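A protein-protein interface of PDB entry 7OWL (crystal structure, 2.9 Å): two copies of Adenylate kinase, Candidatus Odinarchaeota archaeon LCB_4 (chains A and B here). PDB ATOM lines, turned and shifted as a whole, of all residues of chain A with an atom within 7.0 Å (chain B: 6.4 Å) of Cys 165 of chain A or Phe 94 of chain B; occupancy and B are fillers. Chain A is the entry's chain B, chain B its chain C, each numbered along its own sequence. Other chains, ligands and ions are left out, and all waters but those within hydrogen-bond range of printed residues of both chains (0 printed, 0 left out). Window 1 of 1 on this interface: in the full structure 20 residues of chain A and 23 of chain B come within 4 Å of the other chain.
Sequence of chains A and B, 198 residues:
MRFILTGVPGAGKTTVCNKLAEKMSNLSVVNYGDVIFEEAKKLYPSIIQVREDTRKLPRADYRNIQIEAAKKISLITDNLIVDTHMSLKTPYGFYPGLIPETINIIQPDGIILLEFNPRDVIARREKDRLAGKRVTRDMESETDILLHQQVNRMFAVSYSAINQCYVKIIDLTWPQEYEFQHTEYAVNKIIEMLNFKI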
ATOM      1  N   ILE A 103       6.883 -14.720  -3.945  1.00  0.00           N
ATOM      2  CA  ILE A 103       7.571 -14.037  -5.032  1.00  0.00           C
ATOM      3  C   ILE A 103       8.600 -13.055  -4.490  1.00  0.00           C
ATOM      4  O   ILE A 103       9.708 -12.944  -5.028  1.00  0.00           O
ATOM      5  CB  ILE A 103       6.550 -13.347  -5.953  1.00  0.00           C
ATOM      6  CG1 ILE A 103       5.726 -14.406  -6.691  1.00  0.00           C
ATOM      7  CG2 ILE A 103       7.256 -12.413  -6.929  1.00  0.00           C
ATOM      8  CD1 ILE A 103       4.642 -13.839  -7.565  1.00  0.00           C
ATOM      9  N   GLN A 107      12.135 -13.880  -5.267  1.00  0.00           N
ATOM     10  CA  GLN A 107      12.499 -12.759  -6.129  1.00  0.00           C
ATOM     11  C   GLN A 107      12.861 -13.265  -7.531  1.00  0.00           C
ATOM     12  O   GLN A 107      13.953 -12.984  -8.031  1.00  0.00           O
ATOM     13  CB  GLN A 107      13.644 -11.951  -5.527  1.00  0.00           C
ATOM     14  CG  GLN A 107      13.335 -11.374  -4.155  1.00  0.00           C
ATOM     15  CD  GLN A 107      13.408  -9.859  -4.126  1.00  0.00           C
ATOM     16  OE1 GLN A 107      12.991  -9.185  -5.069  1.00  0.00           O
ATOM     17  NE2 GLN A 107      13.944  -9.314  -3.039  1.00  0.00           N
ATOM     18  N   PRO A 108      11.970 -14.010  -8.178  1.00  0.00           N
ATOM     19  CA  PRO A 108      12.288 -14.543  -9.504  1.00  0.00           C
ATOM     20  C   PRO A 108      12.381 -13.436 -10.539  1.00  0.00           C
ATOM     21  O   PRO A 108      11.804 -12.356 -10.397  1.00  0.00           O
ATOM     22  CB  PRO A 108      11.117 -15.484  -9.799  1.00  0.00           C
ATOM     23  CG  PRO A 108       9.988 -14.915  -9.018  1.00  0.00           C
ATOM     24  CD  PRO A 108      10.599 -14.355  -7.763  1.00  0.00           C
ATOM     25  N   ASP A 109      13.134 -13.724 -11.602  1.00  0.00           N
ATOM     26  CA  ASP A 109      13.230 -12.774 -12.704  1.00  0.00           C
ATOM     27  C   ASP A 109      11.957 -12.758 -13.539  1.00  0.00           C
ATOM     28  O   ASP A 109      11.570 -11.700 -14.047  1.00  0.00           O
ATOM     29  CB  ASP A 109      14.434 -13.101 -13.585  1.00  0.00           C
ATOM     30  CG  ASP A 109      15.752 -12.838 -12.890  1.00  0.00           C
ATOM     31  OD1 ASP A 109      15.893 -11.764 -12.265  1.00  0.00           O
ATOM     32  OD2 ASP A 109      16.645 -13.709 -12.963  1.00  0.00           O
ATOM     33  N   GLY A 110      11.286 -13.903 -13.692  1.00  0.00           N
ATOM     34  CA  GLY A 110      10.098 -13.927 -14.522  1.00  0.00           C
ATOM     35  C   GLY A 110       9.124 -15.026 -14.154  1.00  0.00           C
ATOM     36  O   GLY A 110       9.397 -15.886 -13.316  1.00  0.00           O
ATOM     37  N   ILE A 111       7.965 -14.971 -14.807  1.00  0.00           N
ATOM     38  CA  ILE A 111       6.919 -15.982 -14.697  1.00  0.00           C
ATOM     39  C   ILE A 111       6.633 -16.486 -16.103  1.00  0.00           C
ATOM     40  O   ILE A 111       6.301 -15.694 -16.994  1.00  0.00           O
ATOM     41  CB  ILE A 111       5.641 -15.421 -14.051  1.00  0.00           C
ATOM     42  CG1 ILE A 111       5.961 -14.755 -12.709  1.00  0.00           C
ATOM     43  CG2 ILE A 111       4.605 -16.527 -13.858  1.00  0.00           C
ATOM     44  CD1 ILE A 111       4.750 -14.130 -12.032  1.00  0.00           C
ATOM     45  N   ALA A 156      -0.660 -13.938 -13.233  1.00  0.00           N
ATOM     46  CA  ALA A 156       0.734 -13.633 -13.522  1.00  0.00           C
ATOM     47  C   ALA A 156       0.935 -12.138 -13.731  1.00  0.00           C
ATOM     48  O   ALA A 156       1.901 -11.559 -13.222  1.00  0.00           O
ATOM     49  CB  ALA A 156       1.198 -14.413 -14.754  1.00  0.00           C
ATOM     50  N   VAL A 157       0.032 -11.493 -14.472  1.00  0.00           N
ATOM     51  CA  VAL A 157       0.183 -10.064 -14.720  1.00  0.00           C
ATOM     52  C   VAL A 157       0.039  -9.278 -13.423  1.00  0.00           C
ATOM     53  O   VAL A 157       0.725  -8.273 -13.215  1.00  0.00           O
ATOM     54  CB  VAL A 157      -0.822  -9.592 -15.786  1.00  0.00           C
ATOM     55  CG1 VAL A 157      -0.905  -8.068 -15.809  1.00  0.00           C
ATOM     56  CG2 VAL A 157      -0.421 -10.124 -17.152  1.00  0.00           C
ATOM     57  N   TYR A 159       0.829 -10.372 -10.320  1.00  0.00           N
ATOM     58  CA  TYR A 159       2.080 -10.553  -9.590  1.00  0.00           C
ATOM     59  C   TYR A 159       3.200  -9.723 -10.209  1.00  0.00           C
ATOM     60  O   TYR A 159       4.047  -9.176  -9.493  1.00  0.00           O
ATOM     61  CB  TYR A 159       2.465 -12.032  -9.558  1.00  0.00           C
ATOM     62  CG  TYR A 159       1.597 -12.885  -8.657  1.00  0.00           C
ATOM     63  CD1 TYR A 159       1.592 -12.697  -7.282  1.00  0.00           C
ATOM     64  CD2 TYR A 159       0.798 -13.889  -9.181  1.00  0.00           C
ATOM     65  CE1 TYR A 159       0.807 -13.481  -6.457  1.00  0.00           C
ATOM     66  CE2 TYR A 159       0.009 -14.676  -8.366  1.00  0.00           C
ATOM     67  CZ  TYR A 159       0.017 -14.469  -7.007  1.00  0.00           C
ATOM     68  OH  TYR A 159      -0.769 -15.255  -6.196  1.00  0.00           O
ATOM     69  N   SER A 160       3.217  -9.612 -11.538  1.00  0.00           N
ATOM     70  CA  SER A 160       4.240  -8.816 -12.208  1.00  0.00           C
ATOM     71  C   SER A 160       4.092  -7.340 -11.869  1.00  0.00           C
ATOM     72  O   SER A 160       5.068  -6.670 -11.516  1.00  0.00           O
ATOM     73  CB  SER A 160       4.160  -9.030 -13.719  1.00  0.00           C
ATOM     74  OG  SER A 160       4.925  -8.063 -14.414  1.00  0.00           O
ATOM     75  N   ALA A 161       2.872  -6.812 -11.980  1.00  0.00           N
ATOM     76  CA  ALA A 161       2.637  -5.414 -11.642  1.00  0.00           C
ATOM     77  C   ALA A 161       3.026  -5.125 -10.199  1.00  0.00           C
ATOM     78  O   ALA A 161       3.528  -4.039  -9.889  1.00  0.00           O
ATOM     79  CB  ALA A 161       1.170  -5.060 -11.880  1.00  0.00           C
ATOM     80  N   ILE A 162       2.808  -6.088  -9.303  1.00  0.00           N
ATOM     81  CA  ILE A 162       3.105  -5.852  -7.892  1.00  0.00           C
ATOM     82  C   ILE A 162       4.606  -5.917  -7.629  1.00  0.00           C
ATOM     83  O   ILE A 162       5.153  -5.078  -6.903  1.00  0.00           O
ATOM     84  CB  ILE A 162       2.331  -6.857  -7.018  1.00  0.00           C
ATOM     85  CG1 ILE A 162       0.823  -6.628  -7.159  1.00  0.00           C
ATOM     86  CG2 ILE A 162       2.757  -6.727  -5.564  1.00  0.00           C
ATOM     87  CD1 ILE A 162      -0.028  -7.751  -6.599  1.00  0.00           C
ATOM     88  N   ASN A 163       5.296  -6.900  -8.207  1.00  0.00           N
ATOM     89  CA  ASN A 163       6.712  -7.122  -7.946  1.00  0.00           C
ATOM     90  C   ASN A 163       7.610  -6.726  -9.111  1.00  0.00           C
ATOM     91  O   ASN A 163       8.837  -6.811  -8.986  1.00  0.00           O
ATOM     92  CB  ASN A 163       6.953  -8.595  -7.594  1.00  0.00           C
ATOM     93  CG  ASN A 163       6.233  -9.021  -6.324  1.00  0.00           C
ATOM     94  OD1 ASN A 163       6.798  -8.973  -5.231  1.00  0.00           O
ATOM     95  ND2 ASN A 163       4.980  -9.439  -6.466  1.00  0.00           N
ATOM     96  N   GLN A 164       7.039  -6.295 -10.233  1.00  0.00           N
ATOM     97  CA  GLN A 164       7.820  -5.929 -11.409  1.00  0.00           C
ATOM     98  C   GLN A 164       8.734  -7.073 -11.834  1.00  0.00           C
ATOM     99  O   GLN A 164       9.926  -7.082 -11.509  1.00  0.00           O
ATOM    100  CB  GLN A 164       8.639  -4.663 -11.143  1.00  0.00           C
ATOM    101  CG  GLN A 164       8.984  -3.893 -12.414  1.00  0.00           C
ATOM    102  CD  GLN A 164       9.926  -2.730 -12.170  1.00  0.00           C
ATOM    103  OE1 GLN A 164      10.601  -2.666 -11.143  1.00  0.00           O
ATOM    104  NE2 GLN A 164       9.972  -1.801 -13.117  1.00  0.00           N
ATOM    105  N   CYS A 165       8.180  -8.043 -12.559  1.00  0.00           N
ATOM    106  CA  CYS A 165       8.948  -9.147 -13.114  1.00  0.00           C
ATOM    107  C   CYS A 165       8.494  -9.370 -14.551  1.00  0.00           C
ATOM    108  O   CYS A 165       7.603  -8.682 -15.057  1.00  0.00           O
ATOM    109  CB  CYS A 165       8.782 -10.418 -12.271  1.00  0.00           C
ATOM    110  SG  CYS A 165       7.090 -11.041 -12.190  1.00  0.00           S
ATOM    111  N   TYR A 166       9.118 -10.338 -15.216  1.00  0.00           N
ATOM    112  CA  TYR A 166       8.764 -10.648 -16.592  1.00  0.00           C
ATOM    113  C   TYR A 166       7.554 -11.577 -16.638  1.00  0.00           C
ATOM    114  O   TYR A 166       7.278 -12.328 -15.701  1.00  0.00           O
ATOM    115  CB  TYR A 166       9.942 -11.296 -17.321  1.00  0.00           C
ATOM    116  CG  TYR A 166      11.097 -10.356 -17.575  1.00  0.00           C
ATOM    117  CD1 TYR A 166      11.088  -9.493 -18.661  1.00  0.00           C
ATOM    118  CD2 TYR A 166      12.197 -10.334 -16.729  1.00  0.00           C
ATOM    119  CE1 TYR A 166      12.139  -8.633 -18.898  1.00  0.00           C
ATOM    120  CE2 TYR A 166      13.253  -9.479 -16.958  1.00  0.00           C
ATOM    121  CZ  TYR A 166      13.219  -8.629 -18.043  1.00  0.00           C
ATOM    122  OH  TYR A 166      14.269  -7.774 -18.274  1.00  0.00           O
ATOM    123  N   VAL A 167       6.837 -11.531 -17.758  1.00  0.00           N
ATOM    124  CA  VAL A 167       5.685 -12.396 -18.003  1.00  0.00           C
ATOM    125  C   VAL A 167       5.858 -12.986 -19.397  1.00  0.00           C
ATOM    126  O   VAL A 167       5.503 -12.351 -20.396  1.00  0.00           O
ATOM    127  CB  VAL A 167       4.353 -11.648 -17.883  1.00  0.00           C
ATOM    128  CG1 VAL A 167       3.199 -12.554 -18.277  1.00  0.00           C
ATOM    129  CG2 VAL A 167       4.163 -11.129 -16.467  1.00  0.00           C
ATOM    130  N   LYS A 168       6.403 -14.200 -19.470  1.00  0.00           N
ATOM    131  CA  LYS A 168       6.602 -14.911 -20.726  1.00  0.00           C
ATOM    132  C   LYS A 168       5.462 -15.902 -20.919  1.00  0.00           C
ATOM    133  O   LYS A 168       5.124 -16.650 -19.995  1.00  0.00           O
ATOM    134  CB  LYS A 168       7.946 -15.641 -20.723  1.00  0.00           C
ATOM    135  CG  LYS A 168       8.272 -16.416 -21.997  1.00  0.00           C
ATOM    136  CD  LYS A 168       8.703 -15.501 -23.132  1.00  0.00           C
ATOM    137  CE  LYS A 168       9.564 -16.249 -24.141  1.00  0.00           C
ATOM    138  NZ  LYS A 168       9.958 -15.397 -25.300  1.00  0.00           N
ATOM    139  N   ILE A 169       4.872 -15.902 -22.110  1.00  0.00           N
ATOM    140  CA  ILE A 169       3.757 -16.781 -22.447  1.00  0.00           C
ATOM    141  C   ILE A 169       4.217 -17.685 -23.582  1.00  0.00           C
ATOM    142  O   ILE A 169       4.363 -17.231 -24.725  1.00  0.00           O
ATOM    143  CB  ILE A 169       2.502 -15.995 -22.844  1.00  0.00           C
ATOM    144  CG1 ILE A 169       2.057 -15.103 -21.682  1.00  0.00           C
ATOM    145  CG2 ILE A 169       1.386 -16.952 -23.259  1.00  0.00           C
ATOM    146  CD1 ILE A 169       0.897 -14.184 -22.012  1.00  0.00           C
ATOM    147  N   SER B  87       3.670  -2.057 -20.731  1.00  0.00           N
ATOM    148  CA  SER B  87       4.479  -3.263 -20.816  1.00  0.00           C
ATOM    149  C   SER B  87       5.249  -3.247 -22.127  1.00  0.00           C
ATOM    150  O   SER B  87       4.708  -2.870 -23.170  1.00  0.00           O
ATOM    151  CB  SER B  87       3.623  -4.531 -20.724  1.00  0.00           C
ATOM    152  OG  SER B  87       2.950  -4.785 -21.945  1.00  0.00           O
ATOM    153  N   LEU B  88       6.513  -3.650 -22.060  1.00  0.00           N
ATOM    154  CA  LEU B  88       7.357  -3.806 -23.236  1.00  0.00           C
ATOM    155  C   LEU B  88       7.797  -5.258 -23.340  1.00  0.00           C
ATOM    156  O   LEU B  88       8.118  -5.891 -22.328  1.00  0.00           O
ATOM    157  CB  LEU B  88       8.581  -2.891 -23.163  1.00  0.00           C
ATOM    158  CG  LEU B  88       8.293  -1.393 -23.263  1.00  0.00           C
ATOM    159  CD1 LEU B  88       9.069  -0.623 -22.204  1.00  0.00           C
ATOM    160  CD2 LEU B  88       8.632  -0.877 -24.653  1.00  0.00           C
ATOM    161  N   LYS B  89       7.801  -5.790 -24.559  1.00  0.00           N
ATOM    162  CA  LYS B  89       8.196  -7.176 -24.766  1.00  0.00           C
ATOM    163  C   LYS B  89       9.698  -7.273 -24.997  1.00  0.00           C
ATOM    164  O   LYS B  89      10.293  -6.442 -25.690  1.00  0.00           O
ATOM    165  CB  LYS B  89       7.452  -7.807 -25.943  1.00  0.00           C
ATOM    166  CG  LYS B  89       7.698  -9.311 -26.032  1.00  0.00           C
ATOM    167  CD  LYS B  89       6.485 -10.082 -26.543  1.00  0.00           C
ATOM    168  CE  LYS B  89       6.546 -11.567 -26.161  1.00  0.00           C
ATOM    169  NZ  LYS B  89       7.881 -12.019 -25.653  1.00  0.00           N
ATOM    170  N   THR B  90      10.295  -8.308 -24.417  1.00  0.00           N
ATOM    171  CA  THR B  90      11.729  -8.556 -24.446  1.00  0.00           C
ATOM    172  C   THR B  90      11.945 -10.051 -24.655  1.00  0.00           C
ATOM    173  O   THR B  90      10.978 -10.822 -24.605  1.00  0.00           O
ATOM    174  CB  THR B  90      12.370  -8.078 -23.140  1.00  0.00           C
ATOM    175  OG1 THR B  90      11.746  -8.739 -22.031  1.00  0.00           O
ATOM    176  CG2 THR B  90      12.204  -6.571 -22.988  1.00  0.00           C
ATOM    177  N   TYR B  92      12.726 -12.068 -22.633  1.00  0.00           N
ATOM    178  CA  TYR B  92      12.280 -12.723 -21.411  1.00  0.00           C
ATOM    179  C   TYR B  92      10.776 -12.611 -21.192  1.00  0.00           C
ATOM    180  O   TYR B  92      10.268 -13.159 -20.210  1.00  0.00           O
ATOM    181  CB  TYR B  92      13.021 -12.134 -20.205  1.00  0.00           C
ATOM    182  CG  TYR B  92      14.530 -12.196 -20.318  1.00  0.00           C
ATOM    183  CD1 TYR B  92      15.194 -13.415 -20.325  1.00  0.00           C
ATOM    184  CD2 TYR B  92      15.290 -11.035 -20.405  1.00  0.00           C
ATOM    185  CE1 TYR B  92      16.571 -13.477 -20.424  1.00  0.00           C
ATOM    186  CE2 TYR B  92      16.669 -11.089 -20.502  1.00  0.00           C
ATOM    187  CZ  TYR B  92      17.304 -12.314 -20.510  1.00  0.00           C
ATOM    188  OH  TYR B  92      18.676 -12.374 -20.608  1.00  0.00           O
ATOM    189  N   GLY B  93      10.057 -11.919 -22.072  1.00  0.00           N
ATOM    190  CA  GLY B  93       8.621 -11.776 -21.925  1.00  0.00           C
ATOM    191  C   GLY B  93       8.191 -10.333 -21.763  1.00  0.00           C
ATOM    192  O   GLY B  93       8.900  -9.419 -22.186  1.00  0.00           O
ATOM    193  N   PHE B  94       7.029 -10.110 -21.159  1.00  0.00           N
ATOM    194  CA  PHE B  94       6.536  -8.760 -20.940  1.00  0.00           C
ATOM    195  C   PHE B  94       7.102  -8.207 -19.639  1.00  0.00           C
ATOM    196  O   PHE B  94       7.133  -8.900 -18.619  1.00  0.00           O
ATOM    197  CB  PHE B  94       5.008  -8.745 -20.901  1.00  0.00           C
ATOM    198  CG  PHE B  94       4.368  -9.148 -22.196  1.00  0.00           C
ATOM    199  CD1 PHE B  94       4.278  -8.251 -23.246  1.00  0.00           C
ATOM    200  CD2 PHE B  94       3.851 -10.419 -22.362  1.00  0.00           C
ATOM    201  CE1 PHE B  94       3.689  -8.616 -24.437  1.00  0.00           C
ATOM    202  CE2 PHE B  94       3.260 -10.789 -23.551  1.00  0.00           C
ATOM    203  CZ  PHE B  94       3.180  -9.885 -24.590  1.00  0.00           C
ATOM    204  N   TYR B  95       7.552  -6.951 -19.682  1.00  0.00           N
ATOM    205  CA  TYR B  95       8.116  -6.287 -18.518  1.00  0.00           C
ATOM    206  C   TYR B  95       7.373  -4.975 -18.297  1.00  0.00           C
ATOM    207  O   TYR B  95       7.153  -4.222 -19.263  1.00  0.00           O
ATOM    208  CB  TYR B  95       9.615  -6.026 -18.711  1.00  0.00           C
ATOM    209  CG  TYR B  95      10.316  -5.542 -17.464  1.00  0.00           C
ATOM    210  CD1 TYR B  95      10.596  -6.414 -16.422  1.00  0.00           C
ATOM    211  CD2 TYR B  95      10.702  -4.216 -17.331  1.00  0.00           C
ATOM    212  CE1 TYR B  95      11.237  -5.978 -15.280  1.00  0.00           C
ATOM    213  CE2 TYR B  95      11.345  -3.771 -16.193  1.00  0.00           C
ATOM    214  CZ  TYR B  95      11.610  -4.656 -15.171  1.00  0.00           C
ATOM    215  OH  TYR B  95      12.250  -4.218 -14.034  1.00  0.00           O
ATOM    216  N   PRO B  96       6.974  -4.655 -17.065  1.00  0.00           N
ATOM    217  CA  PRO B  96       6.231  -3.413 -16.833  1.00  0.00           C
ATOM    218  C   PRO B  96       7.124  -2.186 -16.886  1.00  0.00           C
ATOM    219  O   PRO B  96       8.308  -2.226 -16.544  1.00  0.00           O
ATOM    220  CB  PRO B  96       5.651  -3.593 -15.422  1.00  0.00           C
ATOM    221  CG  PRO B  96       5.978  -4.995 -15.007  1.00  0.00           C
ATOM    222  CD  PRO B  96       7.156  -5.412 -15.816  1.00  0.00           C
ATOM    223  N   GLU B 140       6.365  -8.748 -35.259  1.00  0.00           N
ATOM    224  CA  GLU B 140       5.240  -9.265 -34.484  1.00  0.00           C
ATOM    225  C   GLU B 140       4.055  -9.609 -35.385  1.00  0.00           C
ATOM    226  O   GLU B 140       3.970  -9.147 -36.523  1.00  0.00           O
ATOM    227  CB  GLU B 140       4.809  -8.253 -33.416  1.00  0.00           C
ATOM    228  CG  GLU B 140       5.606  -8.343 -32.123  1.00  0.00           C
ATOM    229  CD  GLU B 140       5.106  -7.390 -31.052  1.00  0.00           C
ATOM    230  OE1 GLU B 140       3.996  -6.839 -31.211  1.00  0.00           O
ATOM    231  OE2 GLU B 140       5.827  -7.190 -30.052  1.00  0.00           O
ATOM    232  N   ASP B 144       0.308 -11.792 -31.592  1.00  0.00           N
ATOM    233  CA  ASP B 144       1.223 -11.215 -30.612  1.00  0.00           C
ATOM    234  C   ASP B 144       0.771  -9.824 -30.192  1.00  0.00           C
ATOM    235  O   ASP B 144       0.828  -9.475 -29.006  1.00  0.00           O
ATOM    236  CB  ASP B 144       2.637 -11.162 -31.188  1.00  0.00           C
ATOM    237  CG  ASP B 144       3.169 -12.530 -31.552  1.00  0.00           C
ATOM    238  OD1 ASP B 144       2.788 -13.514 -30.881  1.00  0.00           O
ATOM    239  OD2 ASP B 144       3.968 -12.621 -32.508  1.00  0.00           O
ATOM    240  N   LEU B 147      -2.233 -10.076 -27.918  1.00  0.00           N
ATOM    241  CA  LEU B 147      -1.799 -10.518 -26.595  1.00  0.00           C
ATOM    242  C   LEU B 147      -1.143  -9.378 -25.826  1.00  0.00           C
ATOM    243  O   LEU B 147      -1.354  -9.227 -24.615  1.00  0.00           O
ATOM    244  CB  LEU B 147      -0.834 -11.697 -26.731  1.00  0.00           C
ATOM    245  CG  LEU B 147      -0.120 -12.169 -25.461  1.00  0.00           C
ATOM    246  CD1 LEU B 147      -1.105 -12.751 -24.457  1.00  0.00           C
ATOM    247  CD2 LEU B 147       0.959 -13.184 -25.814  1.00  0.00           C
ATOM    248  N   HIS B 148      -0.330  -8.573 -26.511  1.00  0.00           N
ATOM    249  CA  HIS B 148       0.289  -7.430 -25.852  1.00  0.00           C
ATOM    250  C   HIS B 148      -0.768  -6.454 -25.353  1.00  0.00           C
ATOM    251  O   HIS B 148      -0.673  -5.943 -24.231  1.00  0.00           O
ATOM    252  CB  HIS B 148       1.256  -6.737 -26.812  1.00  0.00           C
ATOM    253  CG  HIS B 148       2.168  -5.753 -26.146  1.00  0.00           C
ATOM    254  ND1 HIS B 148       3.115  -5.031 -26.839  1.00  0.00           N
ATOM    255  CD2 HIS B 148       2.276  -5.370 -24.852  1.00  0.00           C
ATOM    256  CE1 HIS B 148       3.768  -4.246 -26.001  1.00  0.00           C
ATOM    257  NE2 HIS B 148       3.278  -4.433 -24.788  1.00  0.00           N
ATOM    258  N   GLN B 149      -1.793  -6.193 -26.165  1.00  0.00           N
ATOM    259  CA  GLN B 149      -2.846  -5.281 -25.730  1.00  0.00           C
ATOM    260  C   GLN B 149      -3.624  -5.862 -24.554  1.00  0.00           C
ATOM    261  O   GLN B 149      -3.996  -5.134 -23.626  1.00  0.00           O
ATOM    262  CB  GLN B 149      -3.780  -4.954 -26.894  1.00  0.00           C
ATOM    263  CG  GLN B 149      -3.084  -4.237 -28.044  1.00  0.00           C
ATOM    264  CD  GLN B 149      -3.978  -3.241 -28.755  1.00  0.00           C
ATOM    265  OE1 GLN B 149      -3.598  -2.085 -28.954  1.00  0.00           O
ATOM    266  NE2 GLN B 149      -5.168  -3.682 -29.152  1.00  0.00           N
ATOM    267  N   VAL B 151      -2.458  -7.947 -22.220  1.00  0.00           N
ATOM    268  CA  VAL B 151      -1.662  -7.865 -20.997  1.00  0.00           C
ATOM    269  C   VAL B 151      -1.522  -6.416 -20.546  1.00  0.00           C
ATOM    270  O   VAL B 151      -1.447  -6.141 -19.343  1.00  0.00           O
ATOM    271  CB  VAL B 151      -0.287  -8.541 -21.175  1.00  0.00           C
ATOM    272  CG1 VAL B 151      -0.461  -9.998 -21.573  1.00  0.00           C
ATOM    273  CG2 VAL B 151       0.562  -7.803 -22.191  1.00  0.00           C
ATOM    274  N   ASN B 152      -1.498  -5.464 -21.483  1.00  0.00           N
ATOM    275  CA  ASN B 152      -1.539  -4.058 -21.090  1.00  0.00           C
ATOM    276  C   ASN B 152      -2.826  -3.744 -20.341  1.00  0.00           C
ATOM    277  O   ASN B 152      -2.804  -3.060 -19.309  1.00  0.00           O
ATOM    278  CB  ASN B 152      -1.411  -3.158 -22.321  1.00  0.00           C
ATOM    279  CG  ASN B 152       0.026  -2.962 -22.758  1.00  0.00           C
ATOM    280  OD1 ASN B 152       0.960  -3.224 -22.003  1.00  0.00           O
ATOM    281  ND2 ASN B 152       0.208  -2.484 -23.980  1.00  0.00           N
ATOM    282  N   PHE B 155      -2.524  -5.156 -16.843  1.00  0.00           N
ATOM    283  CA  PHE B 155      -1.666  -4.311 -16.022  1.00  0.00           C
ATOM    284  C   PHE B 155      -2.414  -3.068 -15.559  1.00  0.00           C
ATOM    285  O   PHE B 155      -2.338  -2.678 -14.388  1.00  0.00           O
ATOM    286  CB  PHE B 155      -0.417  -3.907 -16.803  1.00  0.00           C
ATOM    287  CG  PHE B 155       0.714  -4.892 -16.714  1.00  0.00           C
ATOM    288  CD1 PHE B 155       1.381  -5.096 -15.518  1.00  0.00           C
ATOM    289  CD2 PHE B 155       1.130  -5.591 -17.834  1.00  0.00           C
ATOM    290  CE1 PHE B 155       2.430  -5.993 -15.435  1.00  0.00           C
ATOM    291  CE2 PHE B 155       2.180  -6.489 -17.759  1.00  0.00           C
ATOM    292  CZ  PHE B 155       2.831  -6.690 -16.558  1.00  0.00           C
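The side-chain amide nitrogen (NE2) of Gln 164 of chain A sits close to the side-chain hydroxyl (OH) of Tyr 95 of chain B, 3.4 Å away. O of Phe 94 of chain B sits at hydrogen-bond distance from N of Val 167 of chain A (2.8 Å).
O of Asp 109 of chain A is in hydrogen-bond range of N of Tyr 166 of chain A (3.0 Å). O of Tyr 166 of chain A lies within hydrogen-bond range of N of Ile 111 of chain A (2.9 Å). O of Ile 111 of chain A is in hydrogen-bond range of N of Lys 168 of chain A (2.9 Å). The backbone carbonyl oxygen of Cys 165 of chain A is in hydrogen-bond range of the side-chain hydroxyl of Ser 160 of chain A. O of Leu 88 of chain B lies within hydrogen-bond range of N of Tyr 95 of chain B (2.9 Å). The side-chain hydroxyl (OG1) of Thr 90 of chain B sits at hydrogen-bond distance from the backbone carbonyl oxygen (O) of Gly 93 of chain B (2.9 Å).
OG of Ser 160 of chain A touches CG of Pro 96 of chain B, at 3.3 Å. Ala 161 of chain A touches Phe 155 of chain B (N to CE1, 3.6 Å). Gln 164 of chain A touches Pro 96 of chain B (NE2 to O, 3.8 Å). Phe 94 of chain B touches Cys 165 of chain A (O to O, 3.6 Å). O of Cys 165 of chain A touches CD1 of Tyr 95 of chain B, 3.996 Å away. Cys 165 of chain A touches Pro 96 of chain B (O to CD, 3.4 Å). CE1 of Tyr 166 of chain A touches OG1 of Thr 90 of chain B (3.2 Å). Tyr 166 of chain A touches Tyr 95 of chain B. NZ of Lys 89 of chain B touches NZ of Lys 168 of chain A, 3.98 Å away. Lys 168 of chain A touches Tyr 92 of chain B (CB to O, 3.4 Å).
Of the printed residues of chain B, Cys 165 of chain A touches Phe 94, Tyr 95 and Pro 96. Of chain A, only Cys 165, Tyr 166 and Val 167 come within 4 Å of Phe 94 of chain B. Of the printed residues of chain A, Leu 147 of chain B touches Ile 169 (3.5 Å). Printed residues of chain B within 4 Å of Ser 160 of chain A: Pro 96 and Phe 155. Printed residues of chain B within 4 Å of Lys 168 of chain A: Lys 89, Tyr 92 and Gly 93. The nearest printed residue of chain B that does not touch Cys 165 of chain A is Phe 155 of chain B (5.4 Å).
Hydrophobic or aromatic side chains of chain A that line the printed part of chain B: Val 157, Ala 161, Tyr 166, Val 167 and Ile 169. Of the 17 printed residues of chain B, 9 touch a printed residue of chain A. Printed residues of chain B that touch a printed residue of chain A: Lys 89, Thr 90, Tyr 92, Gly 93, Phe 94, Tyr 95, Pro 96, Leu 147 and Phe 155. Among the printed residues, 19 pairs touch across the chains.
No position is printed for both chains. Of the 19 pairs that touch across the chains among the printed residues, none has its exchanged pair printed and touching as well.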
